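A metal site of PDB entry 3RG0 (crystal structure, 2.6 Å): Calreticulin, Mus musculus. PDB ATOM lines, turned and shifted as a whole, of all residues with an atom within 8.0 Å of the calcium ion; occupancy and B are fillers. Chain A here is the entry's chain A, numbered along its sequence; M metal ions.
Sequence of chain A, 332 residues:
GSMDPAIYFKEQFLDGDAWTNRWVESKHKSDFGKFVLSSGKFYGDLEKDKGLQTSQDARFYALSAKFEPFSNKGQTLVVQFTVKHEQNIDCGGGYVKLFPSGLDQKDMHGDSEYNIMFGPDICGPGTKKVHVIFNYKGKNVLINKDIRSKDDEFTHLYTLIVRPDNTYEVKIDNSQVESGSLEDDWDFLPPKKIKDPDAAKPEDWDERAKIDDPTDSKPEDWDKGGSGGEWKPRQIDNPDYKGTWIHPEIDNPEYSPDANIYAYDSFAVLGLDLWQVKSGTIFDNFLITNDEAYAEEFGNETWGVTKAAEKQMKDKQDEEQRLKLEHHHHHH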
ATOM      1  N   GLU A  11      19.235  24.104  -2.720  1.00  0.00           N
ATOM      2  CA  GLU A  11      19.251  22.860  -1.952  1.00  0.00           C
ATOM      3  C   GLU A  11      20.480  22.821  -1.050  1.00  0.00           C
ATOM      4  O   GLU A  11      21.611  22.919  -1.521  1.00  0.00           O
ATOM      5  CB  GLU A  11      19.210  21.662  -2.896  1.00  0.00           C
ATOM      6  CG  GLU A  11      19.314  20.291  -2.233  1.00  0.00           C
ATOM      7  CD  GLU A  11      18.162  19.967  -1.294  1.00  0.00           C
ATOM      8  OE1 GLU A  11      17.183  19.330  -1.738  1.00  0.00           O
ATOM      9  OE2 GLU A  11      18.233  20.339  -0.096  1.00  0.00           O
ATOM     10  N   GLN A  12      20.235  22.680   0.245  1.00  0.00           N
ATOM     11  CA  GLN A  12      21.306  22.684   1.235  1.00  0.00           C
ATOM     12  C   GLN A  12      21.294  21.469   2.162  1.00  0.00           C
ATOM     13  O   GLN A  12      22.235  21.269   2.925  1.00  0.00           O
ATOM     14  CB  GLN A  12      21.273  23.989   2.049  1.00  0.00           C
ATOM     15  CG  GLN A  12      21.671  25.223   1.268  1.00  0.00           C
ATOM     16  CD  GLN A  12      21.587  26.484   2.104  1.00  0.00           C
ATOM     17  OE1 GLN A  12      20.499  26.936   2.450  1.00  0.00           O
ATOM     18  NE2 GLN A  12      22.743  27.070   2.409  1.00  0.00           N
ATOM     19  N   PHE A  13      20.226  20.665   2.065  1.00  0.00           N
ATOM     20  CA  PHE A  13      20.063  19.427   2.861  1.00  0.00           C
ATOM     21  C   PHE A  13      20.053  19.707   4.362  1.00  0.00           C
ATOM     22  O   PHE A  13      20.907  19.205   5.104  1.00  0.00           O
ATOM     23  CB  PHE A  13      21.135  18.379   2.507  1.00  0.00           C
ATOM     24  CG  PHE A  13      21.361  18.209   1.033  1.00  0.00           C
ATOM     25  CD1 PHE A  13      20.525  17.406   0.262  1.00  0.00           C
ATOM     26  CD2 PHE A  13      22.439  18.834   0.416  1.00  0.00           C
ATOM     27  CE1 PHE A  13      20.748  17.250  -1.103  1.00  0.00           C
ATOM     28  CE2 PHE A  13      22.673  18.687  -0.945  1.00  0.00           C
ATOM     29  CZ  PHE A  13      21.834  17.894  -1.707  1.00  0.00           C
ATOM     30  N   LEU A  14      19.079  20.504   4.806  1.00  0.00           N
ATOM     31  CA  LEU A  14      19.045  21.022   6.178  1.00  0.00           C
ATOM     32  C   LEU A  14      17.943  20.421   7.044  1.00  0.00           C
ATOM     33  O   LEU A  14      17.965  20.569   8.276  1.00  0.00           O
ATOM     34  CB  LEU A  14      18.902  22.553   6.157  1.00  0.00           C
ATOM     35  CG  LEU A  14      19.952  23.398   5.428  1.00  0.00           C
ATOM     36  CD1 LEU A  14      19.481  24.837   5.299  1.00  0.00           C
ATOM     37  CD2 LEU A  14      21.317  23.332   6.114  1.00  0.00           C
ATOM     38  N   LEU A  37      23.188  11.002   2.821  1.00  0.00           N
ATOM     39  CA  LEU A  37      23.324  12.273   3.529  1.00  0.00           C
ATOM     40  C   LEU A  37      24.453  12.191   4.562  1.00  0.00           C
ATOM     41  O   LEU A  37      24.387  11.409   5.512  1.00  0.00           O
ATOM     42  CB  LEU A  37      22.008  12.664   4.219  1.00  0.00           C
ATOM     43  CG  LEU A  37      21.981  14.067   4.851  1.00  0.00           C
ATOM     44  CD1 LEU A  37      21.811  15.132   3.781  1.00  0.00           C
ATOM     45  CD2 LEU A  37      20.884  14.181   5.899  1.00  0.00           C
ATOM     46  N   SER A  38      25.479  13.012   4.361  1.00  0.00           N
ATOM     47  CA  SER A  38      26.676  12.977   5.197  1.00  0.00           C
ATOM     48  C   SER A  38      27.466  14.280   5.126  1.00  0.00           C
ATOM     49  O   SER A  38      27.484  14.952   4.090  1.00  0.00           O
ATOM     50  CB  SER A  38      27.574  11.806   4.769  1.00  0.00           C
ATOM     51  OG  SER A  38      28.687  11.662   5.624  1.00  0.00           O
ATOM     52  N   SER A  39      28.111  14.625   6.239  1.00  0.00           N
ATOM     53  CA  SER A  39      28.987  15.790   6.323  1.00  0.00           C
ATOM     54  C   SER A  39      30.460  15.374   6.376  1.00  0.00           C
ATOM     55  O   SER A  39      31.348  16.220   6.525  1.00  0.00           O
ATOM     56  CB  SER A  39      28.632  16.668   7.525  1.00  0.00           C
ATOM     57  OG  SER A  39      28.549  15.916   8.719  1.00  0.00           O
ATOM     58  N   ASP A  45      30.738  22.657  10.047  1.00  0.00           N
ATOM     59  CA  ASP A  45      29.685  22.423  11.033  1.00  0.00           C
ATOM     60  C   ASP A  45      29.031  21.082  10.734  1.00  0.00           C
ATOM     61  O   ASP A  45      28.679  20.798   9.585  1.00  0.00           O
ATOM     62  CB  ASP A  45      28.650  23.547  10.996  1.00  0.00           C
ATOM     63  CG  ASP A  45      27.533  23.361  12.018  1.00  0.00           C
ATOM     64  OD1 ASP A  45      26.552  22.646  11.717  1.00  0.00           O
ATOM     65  OD2 ASP A  45      27.640  23.940  13.116  1.00  0.00           O
ATOM     66  N   LEU A  46      28.876  20.259  11.766  1.00  0.00           N
ATOM     67  CA  LEU A  46      28.334  18.905  11.625  1.00  0.00           C
ATOM     68  C   LEU A  46      27.024  18.844  10.826  1.00  0.00           C
ATOM     69  O   LEU A  46      26.915  18.096   9.862  1.00  0.00           O
ATOM     70  CB  LEU A  46      28.161  18.258  13.008  1.00  0.00           C
ATOM     71  CG  LEU A  46      27.512  16.874  13.119  1.00  0.00           C
ATOM     72  CD1 LEU A  46      28.332  15.791  12.411  1.00  0.00           C
ATOM     73  CD2 LEU A  46      27.298  16.509  14.592  1.00  0.00           C
ATOM     74  N   GLU A  47      26.050  19.642  11.248  1.00  0.00           N
ATOM     75  CA  GLU A  47      24.718  19.624  10.637  1.00  0.00           C
ATOM     76  C   GLU A  47      24.656  20.359   9.306  1.00  0.00           C
ATOM     77  O   GLU A  47      24.069  19.856   8.344  1.00  0.00           O
ATOM     78  CB  GLU A  47      23.678  20.179  11.615  1.00  0.00           C
ATOM     79  CG  GLU A  47      23.529  19.391  12.913  1.00  0.00           C
ATOM     80  CD  GLU A  47      23.157  17.924  12.697  1.00  0.00           C
ATOM     81  OE1 GLU A  47      22.274  17.646  11.855  1.00  0.00           O
ATOM     82  OE2 GLU A  47      23.746  17.054  13.376  1.00  0.00           O
ATOM     83  N   LYS A  48      25.248  21.550   9.257  1.00  0.00           N
ATOM     84  CA  LYS A  48      25.184  22.425   8.092  1.00  0.00           C
ATOM     85  C   LYS A  48      25.844  21.853   6.841  1.00  0.00           C
ATOM     86  O   LYS A  48      25.270  21.888   5.758  1.00  0.00           O
ATOM     87  CB  LYS A  48      25.774  23.801   8.430  1.00  0.00           C
ATOM     88  CG  LYS A  48      25.661  24.839   7.321  1.00  0.00           C
ATOM     89  CD  LYS A  48      24.238  25.366   7.198  1.00  0.00           C
ATOM     90  CE  LYS A  48      24.178  26.562   6.271  1.00  0.00           C
ATOM     91  NZ  LYS A  48      22.915  27.324   6.466  1.00  0.00           N
ATOM     92  N   ASP A  49      27.058  21.320   6.998  1.00  0.00           N
ATOM     93  CA  ASP A  49      27.825  20.826   5.861  1.00  0.00           C
ATOM     94  C   ASP A  49      27.472  19.390   5.463  1.00  0.00           C
ATOM     95  O   ASP A  49      28.277  18.675   4.867  1.00  0.00           O
ATOM     96  CB  ASP A  49      29.319  20.995   6.100  1.00  0.00           C
ATOM     97  CG  ASP A  49      29.710  22.455   6.265  1.00  0.00           C
ATOM     98  OD1 ASP A  49      29.401  23.263   5.363  1.00  0.00           O
ATOM     99  OD2 ASP A  49      30.299  22.799   7.312  1.00  0.00           O
ATOM    100  N   LYS A  50      26.237  18.984   5.789  1.00  0.00           N
ATOM    101  CA  LYS A  50      25.665  17.738   5.310  1.00  0.00           C
ATOM    102  C   LYS A  50      25.230  17.894   3.849  1.00  0.00           C
ATOM    103  O   LYS A  50      24.586  18.887   3.483  1.00  0.00           O
ATOM    104  CB  LYS A  50      24.480  17.315   6.176  1.00  0.00           C
ATOM    105  CG  LYS A  50      24.885  16.719   7.518  1.00  0.00           C
ATOM    106  CD  LYS A  50      23.665  16.347   8.352  1.00  0.00           C
ATOM    107  CE  LYS A  50      24.073  15.740   9.684  1.00  0.00           C
ATOM    108  NZ  LYS A  50      24.787  14.434   9.522  1.00  0.00           N
ATOM    109  N   GLY A  51      25.604  16.921   3.031  1.00  0.00           N
ATOM    110  CA  GLY A  51      25.227  16.912   1.621  1.00  0.00           C
ATOM    111  C   GLY A  51      25.174  15.514   1.077  1.00  0.00           C
ATOM    112  O   GLY A  51      25.231  14.537   1.838  1.00  0.00           O
ATOM    113  N   LEU A  52      25.063  15.391  -0.236  1.00  0.00           N
ATOM    114  CA  LEU A  52      25.001  14.084  -0.876  1.00  0.00           C
ATOM    115  C   LEU A  52      26.393  13.520  -1.086  1.00  0.00           C
ATOM    116  O   LEU A  52      27.181  14.051  -1.871  1.00  0.00           O
ATOM    117  CB  LEU A  52      24.267  14.165  -2.217  1.00  0.00           C
ATOM    118  CG  LEU A  52      22.813  14.641  -2.181  1.00  0.00           C
ATOM    119  CD1 LEU A  52      22.321  14.900  -3.590  1.00  0.00           C
ATOM    120  CD2 LEU A  52      21.904  13.665  -1.455  1.00  0.00           C
ATOM    121  N   THR A  82      28.755  23.388  -4.278  1.00  0.00           N
ATOM    122  CA  THR A  82      30.054  23.031  -3.701  1.00  0.00           C
ATOM    123  C   THR A  82      30.333  21.551  -3.883  1.00  0.00           C
ATOM    124  O   THR A  82      29.427  20.720  -3.763  1.00  0.00           O
ATOM    125  CB  THR A  82      30.147  23.383  -2.195  1.00  0.00           C
ATOM    126  OG1 THR A  82      29.088  22.739  -1.481  1.00  0.00           O
ATOM    127  CG2 THR A  82      30.060  24.888  -1.977  1.00  0.00           C
ATOM    128  N   ILE A 282      31.232  14.731  -1.565  1.00  0.00           N
ATOM    129  CA  ILE A 282      30.049  15.400  -1.024  1.00  0.00           C
ATOM    130  C   ILE A 282      29.646  16.617  -1.858  1.00  0.00           C
ATOM    131  O   ILE A 282      30.431  17.562  -2.036  1.00  0.00           O
ATOM    132  CB  ILE A 282      30.221  15.818   0.466  1.00  0.00           C
ATOM    133  CG1 ILE A 282      30.707  14.641   1.322  1.00  0.00           C
ATOM    134  CG2 ILE A 282      28.914  16.384   1.018  1.00  0.00           C
ATOM    135  CD1 ILE A 282      31.085  14.999   2.753  1.00  0.00           C
ATOM    136  N   PHE A 283      28.419  16.574  -2.362  1.00  0.00           N
ATOM    137  CA  PHE A 283      27.818  17.706  -3.048  1.00  0.00           C
ATOM    138  C   PHE A 283      26.912  18.450  -2.084  1.00  0.00           C
ATOM    139  O   PHE A 283      26.193  17.834  -1.306  1.00  0.00           O
ATOM    140  CB  PHE A 283      27.008  17.233  -4.249  1.00  0.00           C
ATOM    141  CG  PHE A 283      27.834  16.574  -5.312  1.00  0.00           C
ATOM    142  CD1 PHE A 283      28.071  15.211  -5.284  1.00  0.00           C
ATOM    143  CD2 PHE A 283      28.366  17.332  -6.349  1.00  0.00           C
ATOM    144  CE1 PHE A 283      28.835  14.598  -6.266  1.00  0.00           C
ATOM    145  CE2 PHE A 283      29.127  16.730  -7.344  1.00  0.00           C
ATOM    146  CZ  PHE A 283      29.367  15.356  -7.304  1.00  0.00           C
ATOM    147  N   ASP A 284      26.935  19.772  -2.154  1.00  0.00           N
ATOM    148  CA  ASP A 284      26.193  20.600  -1.213  1.00  0.00           C
ATOM    149  C   ASP A 284      25.881  21.975  -1.803  1.00  0.00           C
ATOM    150  O   ASP A 284      26.493  22.381  -2.805  1.00  0.00           O
ATOM    151  CB  ASP A 284      27.008  20.746   0.080  1.00  0.00           C
ATOM    152  CG  ASP A 284      26.155  21.123   1.294  1.00  0.00           C
ATOM    153  OD1 ASP A 284      24.901  21.139   1.197  1.00  0.00           O
ATOM    154  OD2 ASP A 284      26.768  21.395   2.349  1.00  0.00           O
ATOM    155  N   ASN A 285      24.925  22.669  -1.195  1.00  0.00           N
ATOM    156  CA  ASN A 285      24.628  24.083  -1.478  1.00  0.00           C
ATOM    157  C   ASN A 285      24.428  24.418  -2.949  1.00  0.00           C
ATOM    158  O   ASN A 285      25.111  25.285  -3.510  1.00  0.00           O
ATOM    159  CB  ASN A 285      25.695  24.982  -0.838  1.00  0.00           C
ATOM    160  CG  ASN A 285      25.948  24.653   0.610  1.00  0.00           C
ATOM    161  OD1 ASN A 285      27.067  24.295   0.994  1.00  0.00           O
ATOM    162  ND2 ASN A 285      24.921  24.765   1.440  1.00  0.00           N
ATOM    163  N   PHE A 286      23.490  23.715  -3.582  1.00  0.00           N
ATOM    164  CA  PHE A 286      23.136  23.968  -4.968  1.00  0.00           C
ATOM    165  C   PHE A 286      22.366  25.277  -5.073  1.00  0.00           C
ATOM    166  O   PHE A 286      21.494  25.568  -4.241  1.00  0.00           O
ATOM    167  CB  PHE A 286      22.266  22.833  -5.508  1.00  0.00           C
ATOM    168  CG  PHE A 286      22.966  21.507  -5.558  1.00  0.00           C
ATOM    169  CD1 PHE A 286      23.633  21.101  -6.710  1.00  0.00           C
ATOM    170  CD2 PHE A 286      22.939  20.653  -4.461  1.00  0.00           C
ATOM    171  CE1 PHE A 286      24.277  19.871  -6.762  1.00  0.00           C
ATOM    172  CE2 PHE A 286      23.576  19.417  -4.509  1.00  0.00           C
ATOM    173  CZ  PHE A 286      24.244  19.025  -5.664  1.00  0.00           C
ATOM    174  N   THR A 302      28.001  30.393   2.339  1.00  0.00           N
ATOM    175  CA  THR A 302      27.941  28.940   2.380  1.00  0.00           C
ATOM    176  C   THR A 302      29.335  28.283   2.371  1.00  0.00           C
ATOM    177  O   THR A 302      29.763  27.745   3.388  1.00  0.00           O
ATOM    178  CB  THR A 302      26.945  28.382   1.300  1.00  0.00           C
ATOM    179  OG1 THR A 302      26.351  27.169   1.756  1.00  0.00           O
ATOM    180  CG2 THR A 302      27.587  28.195  -0.075  1.00  0.00           C
ATOM    181  N   THR A 306      32.280  27.636   5.498  1.00  0.00           N
ATOM    182  CA  THR A 306      32.762  26.267   5.671  1.00  0.00           C
ATOM    183  C   THR A 306      34.295  26.187   5.702  1.00  0.00           C
ATOM    184  O   THR A 306      34.868  25.621   6.632  1.00  0.00           O
ATOM    185  CB  THR A 306      32.219  25.332   4.556  1.00  0.00           C
ATOM    186  OG1 THR A 306      30.791  25.296   4.623  1.00  0.00           O
ATOM    187  CG2 THR A 306      32.758  23.909   4.697  1.00  0.00           C
HETATM  188 CA    CA M   1      24.425  21.336   3.769  1.00  0.00          CA
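The backbone NH (N) of Lys 48 lies within hydrogen-bond range of the side-chain carboxylate (OD1) of Asp 45 (3.0 Å).
ND2 of Asn 285 sits close to NE2 of Gln 12 (3.3 Å).
The side-chain amide oxygen of Asn 285 lies close to the side-chain carboxylate of Asp 284.
The backbone carbonyl oxygen (O) of Asp 284 is in hydrogen-bond range of the backbone NH (N) of Thr 82 (2.9 Å).
The side-chain carboxylate of Asp 49 lies within hydrogen-bond range of the backbone NH of Asp 45, 2.8 Å away.
The side-chain carboxylate of Asp 49 sits at hydrogen-bond distance from the side-chain hydroxyl of Thr 306 (2.6 Å).
C of Asp 49 touches the calcium ion, 3.99 Å away.
Of the 23 residues printed, 5 come within 4 Å of the calcium ion.
The calcium ion is bound by O of Lys 48 (2.2 Å), O of Gln 12 (2.3 Å), O of Lys 50 (2.5 Å), OD1 of Asp 284 (2.6 Å) and OD2 of Asp 284 (2.7 Å).
The calcium ion has five donor atoms within binding distance.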
